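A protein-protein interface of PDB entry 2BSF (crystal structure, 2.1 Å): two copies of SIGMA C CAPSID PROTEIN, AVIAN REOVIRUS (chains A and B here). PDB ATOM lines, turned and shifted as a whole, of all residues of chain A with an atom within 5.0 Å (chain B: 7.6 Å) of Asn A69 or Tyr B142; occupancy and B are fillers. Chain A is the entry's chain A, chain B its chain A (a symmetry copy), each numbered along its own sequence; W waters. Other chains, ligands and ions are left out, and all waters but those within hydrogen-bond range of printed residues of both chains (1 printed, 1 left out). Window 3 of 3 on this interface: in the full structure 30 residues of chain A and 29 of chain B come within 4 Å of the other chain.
ND2 of Asn A69 sits close to OH of Tyr B142 (3.5 Å).
A ring nitrogen (NE2) of His A71 sits close to the backbone carbonyl oxygen of Ser B123 (3.5 Å).
No position is printed for both chains.
Of the 9 pairs that touch across the chains among the printed residues, none has its exchanged pair printed and touching as well.
O of Asn A69 lies within hydrogen-bond range of N of Met A80 (2.9 Å).
The backbone NH (N) of His A71 lies within hydrogen-bond range of the backbone carbonyl oxygen (O) of Asp A78, at 2.8 Å.
The backbone NH of Gly B143 lies within hydrogen-bond range of the backbone carbonyl oxygen of Phe B124, at 2.8 Å.
O of Pro B125 sits at hydrogen-bond distance from OG1 of Thr B172 (2.6 Å).
N of Val B126 lies close to NE2 of Gln B140 (3.4 Å).
The backbone carbonyl oxygen (O) of Tyr B142 is in hydrogen-bond range of the backbone NH (N) of Thr B154, at 3.2 Å.
Among the printed residues, merely in contact across the chains: Leu A47 with Ser B123, Leu A47 with Tyr B142, His A71 with Phe B124, His A71 with Pro B125, Met A80 with Pro B125, Met A80 with Gln B140 and Met A80 with Tyr B142.
Hydrophobic or aromatic side chains of chain A that line the printed part of chain B: Leu A47, His A71 and Met A80.
Of the 20 printed residues of chain B, 5 touch a printed residue of chain A.
Among the printed residues, 9 pairs touch across the chains.
Among the printed residues, no Asp or Glu carboxylate lies within 4 Å of a Lys or Arg side-chain nitrogen of the other chain.
Water W1 lies within hydrogen-bond range of the side-chain amide oxygen (OE1) of Gln B140 and the side-chain sulfur (SD) of Met A80.
Of chain B, only Tyr B142 comes within 4 Å of Asn A69.
Of the printed residues of chain B, His A71 touches Ser B123 (3.2 Å), Phe B124 (3.7 Å) and Pro B125 (3.4 Å).
Of the printed residues of chain A, Pro B125 touches His A71 (3.4 Å) and Met A80 (3.6 Å).
Tyr B142 touches three residues of chain A.
The nearest printed residue of chain A that does not touch Tyr B142 is His A71 (5.8 Å).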
ATOM      1  N   LEU A  47      -4.003  25.149   1.049  1.00  0.00           N
ATOM      2  CA  LEU A  47      -5.374  24.711   0.865  1.00  0.00           C
ATOM      3  C   LEU A  47      -5.754  25.200  -0.523  1.00  0.00           C
ATOM      4  O   LEU A  47      -5.942  26.389  -0.738  1.00  0.00           O
ATOM      5  CB  LEU A  47      -6.302  25.286   1.954  1.00  0.00           C
ATOM      6  CG  LEU A  47      -7.782  24.853   1.887  1.00  0.00           C
ATOM      7  CD1 LEU A  47      -7.889  23.349   2.193  1.00  0.00           C
ATOM      8  CD2 LEU A  47      -8.624  25.657   2.878  1.00  0.00           C
ATOM      9  N   MET A  48      -5.785  24.271  -1.472  1.00  0.00           N
ATOM     10  CA  MET A  48      -6.103  24.560  -2.877  1.00  0.00           C
ATOM     11  C   MET A  48      -7.606  24.374  -3.032  1.00  0.00           C
ATOM     12  O   MET A  48      -8.191  23.511  -2.389  1.00  0.00           O
ATOM     13  CB  MET A  48      -5.376  23.578  -3.800  1.00  0.00           C
ATOM     14  CG  MET A  48      -3.864  23.499  -3.655  1.00  0.00           C
ATOM     15  SD  MET A  48      -3.197  22.163  -4.703  1.00  0.00           S
ATOM     16  CE  MET A  48      -1.455  22.356  -4.368  1.00  0.00           C
ATOM     17  N   GLN A  49      -8.232  25.219  -3.846  1.00  0.00           N
ATOM     18  CA  GLN A  49      -9.657  25.152  -4.099  1.00  0.00           C
ATOM     19  C   GLN A  49      -9.829  25.196  -5.589  1.00  0.00           C
ATOM     20  O   GLN A  49      -9.323  26.082  -6.250  1.00  0.00           O
ATOM     21  CB  GLN A  49     -10.375  26.354  -3.499  1.00  0.00           C
ATOM     22  CG  GLN A  49     -10.129  26.541  -2.002  1.00  0.00           C
ATOM     23  CD  GLN A  49     -10.946  27.673  -1.428  1.00  0.00           C
ATOM     24  OE1 GLN A  49     -10.402  28.677  -0.983  1.00  0.00           O
ATOM     25  NE2 GLN A  49     -12.265  27.530  -1.468  1.00  0.00           N
ATOM     26  N   THR A  67     -16.668  20.512  -6.368  1.00  0.00           N
ATOM     27  CA  THR A  67     -15.939  21.589  -5.734  1.00  0.00           C
ATOM     28  C   THR A  67     -14.970  20.916  -4.764  1.00  0.00           C
ATOM     29  O   THR A  67     -15.393  20.169  -3.869  1.00  0.00           O
ATOM     30  CB  THR A  67     -16.903  22.504  -4.955  1.00  0.00           C
ATOM     31  OG1 THR A  67     -17.750  23.163  -5.902  1.00  0.00           O
ATOM     32  CG2 THR A  67     -16.127  23.545  -4.138  1.00  0.00           C
ATOM     33  N   VAL A  68     -13.675  21.160  -4.983  1.00  0.00           N
ATOM     34  CA  VAL A  68     -12.619  20.453  -4.268  1.00  0.00           C
ATOM     35  C   VAL A  68     -11.815  21.423  -3.416  1.00  0.00           C
ATOM     36  O   VAL A  68     -11.401  22.489  -3.866  1.00  0.00           O
ATOM     37  CB  VAL A  68     -11.685  19.649  -5.240  1.00  0.00           C
ATOM     38  CG1 VAL A  68     -10.641  18.826  -4.499  1.00  0.00           C
ATOM     39  CG2 VAL A  68     -12.473  18.717  -6.123  1.00  0.00           C
ATOM     40  N   ASN A  69     -11.597  21.039  -2.174  1.00  0.00           N
ATOM     41  CA  ASN A  69     -10.545  21.617  -1.380  1.00  0.00           C
ATOM     42  C   ASN A  69      -9.523  20.533  -1.156  1.00  0.00           C
ATOM     43  O   ASN A  69      -9.867  19.439  -0.697  1.00  0.00           O
ATOM     44  CB  ASN A  69     -11.094  22.096  -0.040  1.00  0.00           C
ATOM     45  CG  ASN A  69     -11.726  23.488  -0.147  1.00  0.00           C
ATOM     46  OD1 ASN A  69     -11.047  24.498  -0.061  1.00  0.00           O
ATOM     47  ND2 ASN A  69     -13.010  23.526  -0.342  1.00  0.00           N
ATOM     48  N   ALA A  70      -8.279  20.847  -1.474  1.00  0.00           N
ATOM     49  CA  ALA A  70      -7.167  19.931  -1.279  1.00  0.00           C
ATOM     50  C   ALA A  70      -6.264  20.552  -0.250  1.00  0.00           C
ATOM     51  O   ALA A  70      -5.665  21.598  -0.497  1.00  0.00           O
ATOM     52  CB  ALA A  70      -6.432  19.684  -2.602  1.00  0.00           C
ATOM     53  N   HIS A  71      -6.222  19.953   0.939  1.00  0.00           N
ATOM     54  CA  HIS A  71      -5.336  20.434   1.997  1.00  0.00           C
ATOM     55  C   HIS A  71      -4.021  19.661   1.913  1.00  0.00           C
ATOM     56  O   HIS A  71      -3.987  18.445   2.171  1.00  0.00           O
ATOM     57  CB  HIS A  71      -5.992  20.253   3.374  1.00  0.00           C
ATOM     58  CG  HIS A  71      -5.142  20.738   4.508  1.00  0.00           C
ATOM     59  ND1 HIS A  71      -4.808  19.947   5.596  1.00  0.00           N
ATOM     60  CD2 HIS A  71      -4.560  21.940   4.726  1.00  0.00           C
ATOM     61  CE1 HIS A  71      -4.079  20.651   6.441  1.00  0.00           C
ATOM     62  NE2 HIS A  71      -3.905  21.862   5.932  1.00  0.00           N
ATOM     63  N   ASP A  78      -5.022  15.905   1.458  1.00  0.00           N
ATOM     64  CA  ASP A  78      -6.395  15.455   1.775  1.00  0.00           C
ATOM     65  C   ASP A  78      -7.431  16.180   0.935  1.00  0.00           C
ATOM     66  O   ASP A  78      -7.379  17.395   0.828  1.00  0.00           O
ATOM     67  CB  ASP A  78      -6.658  15.647   3.243  1.00  0.00           C
ATOM     68  CG  ASP A  78      -5.712  14.823   4.096  1.00  0.00           C
ATOM     69  OD1 ASP A  78      -5.688  13.606   3.886  1.00  0.00           O
ATOM     70  OD2 ASP A  78      -5.009  15.374   4.977  1.00  0.00           O
ATOM     71  N   TYR A  79      -8.358  15.420   0.342  1.00  0.00           N
ATOM     72  CA  TYR A  79      -9.400  15.970  -0.527  1.00  0.00           C
ATOM     73  C   TYR A  79     -10.736  15.989   0.161  1.00  0.00           C
ATOM     74  O   TYR A  79     -11.133  15.006   0.802  1.00  0.00           O
ATOM     75  CB  TYR A  79      -9.603  15.104  -1.755  1.00  0.00           C
ATOM     76  CG  TYR A  79      -8.509  15.125  -2.791  1.00  0.00           C
ATOM     77  CD1 TYR A  79      -8.057  16.330  -3.363  1.00  0.00           C
ATOM     78  CD2 TYR A  79      -7.996  13.918  -3.289  1.00  0.00           C
ATOM     79  CE1 TYR A  79      -7.070  16.326  -4.378  1.00  0.00           C
ATOM     80  CE2 TYR A  79      -7.029  13.905  -4.294  1.00  0.00           C
ATOM     81  CZ  TYR A  79      -6.578  15.106  -4.843  1.00  0.00           C
ATOM     82  OH  TYR A  79      -5.617  15.056  -5.843  1.00  0.00           O
ATOM     83  N   MET A  80     -11.420  17.123   0.028  1.00  0.00           N
ATOM     84  CA  MET A  80     -12.772  17.266   0.487  1.00  0.00           C
ATOM     85  C   MET A  80     -13.521  17.753  -0.751  1.00  0.00           C
ATOM     86  O   MET A  80     -13.249  18.836  -1.245  1.00  0.00           O
ATOM     87  CB  MET A  80     -12.819  18.339   1.568  1.00  0.00           C
ATOM     88  CG  MET A  80     -12.142  18.007   2.944  1.00  0.00           C
ATOM     89  SD  MET A  80     -10.310  17.861   3.054  1.00  0.00           S
ATOM     90  CE  MET A  80      -9.750  19.549   2.735  1.00  0.00           C
ATOM     91  N   VAL B  94     -20.436  31.738  12.598  1.00  0.00           N
ATOM     92  CA  VAL B  94     -19.742  32.063  13.852  1.00  0.00           C
ATOM     93  C   VAL B  94     -18.258  31.741  13.703  1.00  0.00           C
ATOM     94  O   VAL B  94     -17.877  30.819  12.951  1.00  0.00           O
ATOM     95  CB  VAL B  94     -20.416  31.354  15.084  1.00  0.00           C
ATOM     96  CG1 VAL B  94     -20.339  29.850  14.902  1.00  0.00           C
ATOM     97  CG2 VAL B  94     -19.793  31.819  16.422  1.00  0.00           C
ATOM     98  N   LEU B  96     -15.068  30.809  16.121  1.00  0.00           N
ATOM     99  CA  LEU B  96     -14.773  30.266  17.444  1.00  0.00           C
ATOM    100  C   LEU B  96     -13.286  30.043  17.584  1.00  0.00           C
ATOM    101  O   LEU B  96     -12.672  29.309  16.817  1.00  0.00           O
ATOM    102  CB  LEU B  96     -15.546  28.969  17.672  1.00  0.00           C
ATOM    103  CG  LEU B  96     -15.761  28.464  19.089  1.00  0.00           C
ATOM    104  CD1 LEU B  96     -16.592  29.446  19.997  1.00  0.00           C
ATOM    105  CD2 LEU B  96     -16.433  27.085  18.938  1.00  0.00           C
ATOM    106  N   SER B 123      -5.078  27.458   5.979  1.00  0.00           N
ATOM    107  CA  SER B 123      -6.317  26.973   6.549  1.00  0.00           C
ATOM    108  C   SER B 123      -6.310  25.445   6.527  1.00  0.00           C
ATOM    109  O   SER B 123      -5.675  24.814   5.675  1.00  0.00           O
ATOM    110  CB  SER B 123      -7.523  27.543   5.786  1.00  0.00           C
ATOM    111  OG  SER B 123      -7.649  28.946   6.018  1.00  0.00           O
ATOM    112  N   PHE B 124      -6.980  24.850   7.501  1.00  0.00           N
ATOM    113  CA  PHE B 124      -6.977  23.391   7.667  1.00  0.00           C
ATOM    114  C   PHE B 124      -8.397  22.895   7.924  1.00  0.00           C
ATOM    115  O   PHE B 124      -9.202  23.626   8.505  1.00  0.00           O
ATOM    116  CB  PHE B 124      -5.988  22.961   8.788  1.00  0.00           C
ATOM    117  CG  PHE B 124      -6.245  23.605  10.133  1.00  0.00           C
ATOM    118  CD1 PHE B 124      -5.701  24.848  10.441  1.00  0.00           C
ATOM    119  CD2 PHE B 124      -7.029  22.958  11.085  1.00  0.00           C
ATOM    120  CE1 PHE B 124      -5.944  25.442  11.687  1.00  0.00           C
ATOM    121  CE2 PHE B 124      -7.264  23.520  12.332  1.00  0.00           C
ATOM    122  CZ  PHE B 124      -6.728  24.785  12.630  1.00  0.00           C
ATOM    123  N   PRO B 125      -8.724  21.674   7.469  1.00  0.00           N
ATOM    124  CA  PRO B 125     -10.121  21.215   7.658  1.00  0.00           C
ATOM    125  C   PRO B 125     -10.469  20.825   9.085  1.00  0.00           C
ATOM    126  O   PRO B 125      -9.632  20.312   9.848  1.00  0.00           O
ATOM    127  CB  PRO B 125     -10.287  20.046   6.660  1.00  0.00           C
ATOM    128  CG  PRO B 125      -8.887  19.624   6.271  1.00  0.00           C
ATOM    129  CD  PRO B 125      -7.897  20.714   6.711  1.00  0.00           C
ATOM    130  N   VAL B 126     -11.707  21.147   9.443  1.00  0.00           N
ATOM    131  CA  VAL B 126     -12.261  20.898  10.750  1.00  0.00           C
ATOM    132  C   VAL B 126     -13.688  20.366  10.554  1.00  0.00           C
ATOM    133  O   VAL B 126     -14.461  20.992   9.846  1.00  0.00           O
ATOM    134  CB  VAL B 126     -12.315  22.226  11.556  1.00  0.00           C
ATOM    135  CG1 VAL B 126     -12.981  22.006  12.906  1.00  0.00           C
ATOM    136  CG2 VAL B 126     -10.885  22.793  11.748  1.00  0.00           C
ATOM    137  N   ASP B 127     -14.014  19.221  11.158  1.00  0.00           N
ATOM    138  CA  ASP B 127     -15.374  18.705  11.095  1.00  0.00           C
ATOM    139  C   ASP B 127     -16.117  19.293  12.276  1.00  0.00           C
ATOM    140  O   ASP B 127     -15.657  19.184  13.438  1.00  0.00           O
ATOM    141  CB  ASP B 127     -15.408  17.183  11.209  1.00  0.00           C
ATOM    142  CG  ASP B 127     -14.954  16.479   9.901  1.00  0.00           C
ATOM    143  OD1 ASP B 127     -14.692  17.160   8.888  1.00  0.00           O
ATOM    144  OD2 ASP B 127     -14.904  15.247   9.873  1.00  0.00           O
ATOM    145  N   VAL B 128     -17.262  19.909  11.994  1.00  0.00           N
ATOM    146  CA  VAL B 128     -18.054  20.534  13.072  1.00  0.00           C
ATOM    147  C   VAL B 128     -19.491  19.978  13.027  1.00  0.00           C
ATOM    148  O   VAL B 128     -20.026  19.779  11.958  1.00  0.00           O
ATOM    149  CB  VAL B 128     -18.097  22.057  12.832  1.00  0.00           C
ATOM    150  CG1 VAL B 128     -19.028  22.734  13.827  1.00  0.00           C
ATOM    151  CG2 VAL B 128     -16.694  22.632  12.976  1.00  0.00           C
ATOM    152  N   TYR B 139     -20.932  20.090   9.179  1.00  0.00           N
ATOM    153  CA  TYR B 139     -20.206  20.813   8.144  1.00  0.00           C
ATOM    154  C   TYR B 139     -18.728  20.419   8.142  1.00  0.00           C
ATOM    155  O   TYR B 139     -18.130  20.201   9.213  1.00  0.00           O
ATOM    156  CB  TYR B 139     -20.228  22.314   8.437  1.00  0.00           C
ATOM    157  CG  TYR B 139     -21.593  22.910   8.583  1.00  0.00           C
ATOM    158  CD1 TYR B 139     -22.379  23.205   7.450  1.00  0.00           C
ATOM    159  CD2 TYR B 139     -22.118  23.180   9.854  1.00  0.00           C
ATOM    160  CE1 TYR B 139     -23.659  23.765   7.592  1.00  0.00           C
ATOM    161  CE2 TYR B 139     -23.391  23.721  10.002  1.00  0.00           C
ATOM    162  CZ  TYR B 139     -24.143  24.025   8.879  1.00  0.00           C
ATOM    163  OH  TYR B 139     -25.381  24.560   9.039  1.00  0.00           O
ATOM    164  N   GLN B 140     -18.165  20.339   6.939  1.00  0.00           N
ATOM    165  CA  GLN B 140     -16.726  20.389   6.718  1.00  0.00           C
ATOM    166  C   GLN B 140     -16.405  21.883   6.855  1.00  0.00           C
ATOM    167  O   GLN B 140     -16.769  22.656   5.986  1.00  0.00           O
ATOM    168  CB  GLN B 140     -16.404  19.910   5.290  1.00  0.00           C
ATOM    169  CG  GLN B 140     -14.951  20.149   4.823  1.00  0.00           C
ATOM    170  CD  GLN B 140     -13.994  19.478   5.732  1.00  0.00           C
ATOM    171  OE1 GLN B 140     -13.817  18.268   5.679  1.00  0.00           O
ATOM    172  NE2 GLN B 140     -13.372  20.253   6.595  1.00  0.00           N
ATOM    173  N   ALA B 141     -15.797  22.298   7.965  1.00  0.00           N
ATOM    174  CA  ALA B 141     -15.426  23.714   8.151  1.00  0.00           C
ATOM    175  C   ALA B 141     -13.915  23.864   7.997  1.00  0.00           C
ATOM    176  O   ALA B 141     -13.255  22.894   7.681  1.00  0.00           O
ATOM    177  CB  ALA B 141     -15.924  24.228   9.543  1.00  0.00           C
ATOM    178  N   TYR B 142     -13.366  25.057   8.240  1.00  0.00           N
ATOM    179  CA  TYR B 142     -11.908  25.305   8.184  1.00  0.00           C
ATOM    180  C   TYR B 142     -11.461  26.138   9.378  1.00  0.00           C
ATOM    181  O   TYR B 142     -12.218  26.933   9.910  1.00  0.00           O
ATOM    182  CB  TYR B 142     -11.495  25.948   6.832  1.00  0.00           C
ATOM    183  CG  TYR B 142     -11.728  24.948   5.701  1.00  0.00           C
ATOM    184  CD1 TYR B 142     -10.739  23.994   5.366  1.00  0.00           C
ATOM    185  CD2 TYR B 142     -12.963  24.879   5.040  1.00  0.00           C
ATOM    186  CE1 TYR B 142     -10.968  23.000   4.349  1.00  0.00           C
ATOM    187  CE2 TYR B 142     -13.216  23.879   4.030  1.00  0.00           C
ATOM    188  CZ  TYR B 142     -12.207  22.957   3.705  1.00  0.00           C
ATOM    189  OH  TYR B 142     -12.439  21.995   2.732  1.00  0.00           O
ATOM    190  N   GLY B 143     -10.227  25.931   9.798  1.00  0.00           N
ATOM    191  CA  GLY B 143      -9.645  26.669  10.917  1.00  0.00           C
ATOM    192  C   GLY B 143      -8.446  27.355  10.324  1.00  0.00           C
ATOM    193  O   GLY B 143      -8.032  26.993   9.234  1.00  0.00           O
ATOM    194  N   VAL B 144      -7.923  28.359  11.008  1.00  0.00           N
ATOM    195  CA  VAL B 144      -6.654  28.998  10.605  1.00  0.00           C
ATOM    196  C   VAL B 144      -5.940  29.516  11.861  1.00  0.00           C
ATOM    197  O   VAL B 144      -6.579  30.071  12.740  1.00  0.00           O
ATOM    198  CB  VAL B 144      -6.844  30.121   9.520  1.00  0.00           C
ATOM    199  CG1 VAL B 144      -7.679  31.293  10.032  1.00  0.00           C
ATOM    200  CG2 VAL B 144      -5.460  30.611   8.940  1.00  0.00           C
ATOM    201  N   PHE B 151      -5.894  29.438  17.103  1.00  0.00           N
ATOM    202  CA  PHE B 151      -6.594  29.234  15.834  1.00  0.00           C
ATOM    203  C   PHE B 151      -8.065  29.555  15.997  1.00  0.00           C
ATOM    204  O   PHE B 151      -8.616  29.555  17.114  1.00  0.00           O
ATOM    205  CB  PHE B 151      -6.400  27.816  15.267  1.00  0.00           C
ATOM    206  CG  PHE B 151      -7.069  26.704  16.058  1.00  0.00           C
ATOM    207  CD1 PHE B 151      -6.401  26.062  17.097  1.00  0.00           C
ATOM    208  CD2 PHE B 151      -8.315  26.227  15.690  1.00  0.00           C
ATOM    209  CE1 PHE B 151      -6.964  25.005  17.788  1.00  0.00           C
ATOM    210  CE2 PHE B 151      -8.895  25.169  16.376  1.00  0.00           C
ATOM    211  CZ  PHE B 151      -8.228  24.562  17.434  1.00  0.00           C
ATOM    212  N   THR B 152      -8.697  29.819  14.875  1.00  0.00           N
ATOM    213  CA  THR B 152     -10.099  30.176  14.876  1.00  0.00           C
ATOM    214  C   THR B 152     -10.760  29.321  13.820  1.00  0.00           C
ATOM    215  O   THR B 152     -10.224  29.194  12.720  1.00  0.00           O
ATOM    216  CB  THR B 152     -10.266  31.676  14.535  1.00  0.00           C
ATOM    217  OG1 THR B 152      -9.655  32.425  15.582  1.00  0.00           O
ATOM    218  CG2 THR B 152     -11.744  32.079  14.452  1.00  0.00           C
ATOM    219  N   ILE B 153     -11.917  28.741  14.150  1.00  0.00           N
ATOM    220  CA  ILE B 153     -12.678  28.032  13.145  1.00  0.00           C
ATOM    221  C   ILE B 153     -13.900  28.872  12.777  1.00  0.00           C
ATOM    222  O   ILE B 153     -14.451  29.609  13.602  1.00  0.00           O
ATOM    223  CB  ILE B 153     -13.051  26.584  13.597  1.00  0.00           C
ATOM    224  CG1 ILE B 153     -14.025  26.603  14.794  1.00  0.00           C
ATOM    225  CG2 ILE B 153     -11.760  25.828  13.995  1.00  0.00           C
ATOM    226  CD1 ILE B 153     -14.531  25.152  15.266  1.00  0.00           C
ATOM    227  N   THR B 154     -14.313  28.746  11.535  1.00  0.00           N
ATOM    228  CA  THR B 154     -15.468  29.469  11.026  1.00  0.00           C
ATOM    229  C   THR B 154     -16.471  28.436  10.554  1.00  0.00           C
ATOM    230  O   THR B 154     -16.129  27.543   9.764  1.00  0.00           O
ATOM    231  CB  THR B 154     -15.024  30.327   9.835  1.00  0.00           C
ATOM    232  OG1 THR B 154     -14.043  31.267  10.287  1.00  0.00           O
ATOM    233  CG2 THR B 154     -16.198  31.033   9.180  1.00  0.00           C
ATOM    234  N   PHE B 155     -17.713  28.542  11.028  1.00  0.00           N
ATOM    235  CA  PHE B 155     -18.722  27.614  10.585  1.00  0.00           C
ATOM    236  C   PHE B 155     -20.137  28.235  10.581  1.00  0.00           C
ATOM    237  O   PHE B 155     -20.406  29.240  11.283  1.00  0.00           O
ATOM    238  CB  PHE B 155     -18.638  26.271  11.360  1.00  0.00           C
ATOM    239  CG  PHE B 155     -18.823  26.405  12.871  1.00  0.00           C
ATOM    240  CD1 PHE B 155     -17.720  26.615  13.699  1.00  0.00           C
ATOM    241  CD2 PHE B 155     -20.091  26.318  13.450  1.00  0.00           C
ATOM    242  CE1 PHE B 155     -17.875  26.757  15.085  1.00  0.00           C
ATOM    243  CE2 PHE B 155     -20.262  26.433  14.839  1.00  0.00           C
ATOM    244  CZ  PHE B 155     -19.147  26.642  15.657  1.00  0.00           C
ATOM    245  N   THR B 172     -10.472  17.672  14.363  1.00  0.00           N
ATOM    246  CA  THR B 172      -9.450  18.183  13.445  1.00  0.00           C
ATOM    247  C   THR B 172      -8.081  17.677  13.942  1.00  0.00           C
ATOM    248  O   THR B 172      -7.998  16.983  14.964  1.00  0.00           O
ATOM    249  CB  THR B 172      -9.466  19.751  13.361  1.00  0.00           C
ATOM    250  OG1 THR B 172      -8.649  20.196  12.272  1.00  0.00           O
ATOM    251  CG2 THR B 172      -8.959  20.395  14.640  1.00  0.00           C
HETATM  252  O   HOH W   1     -11.316  16.582   6.252  1.00  0.00           O
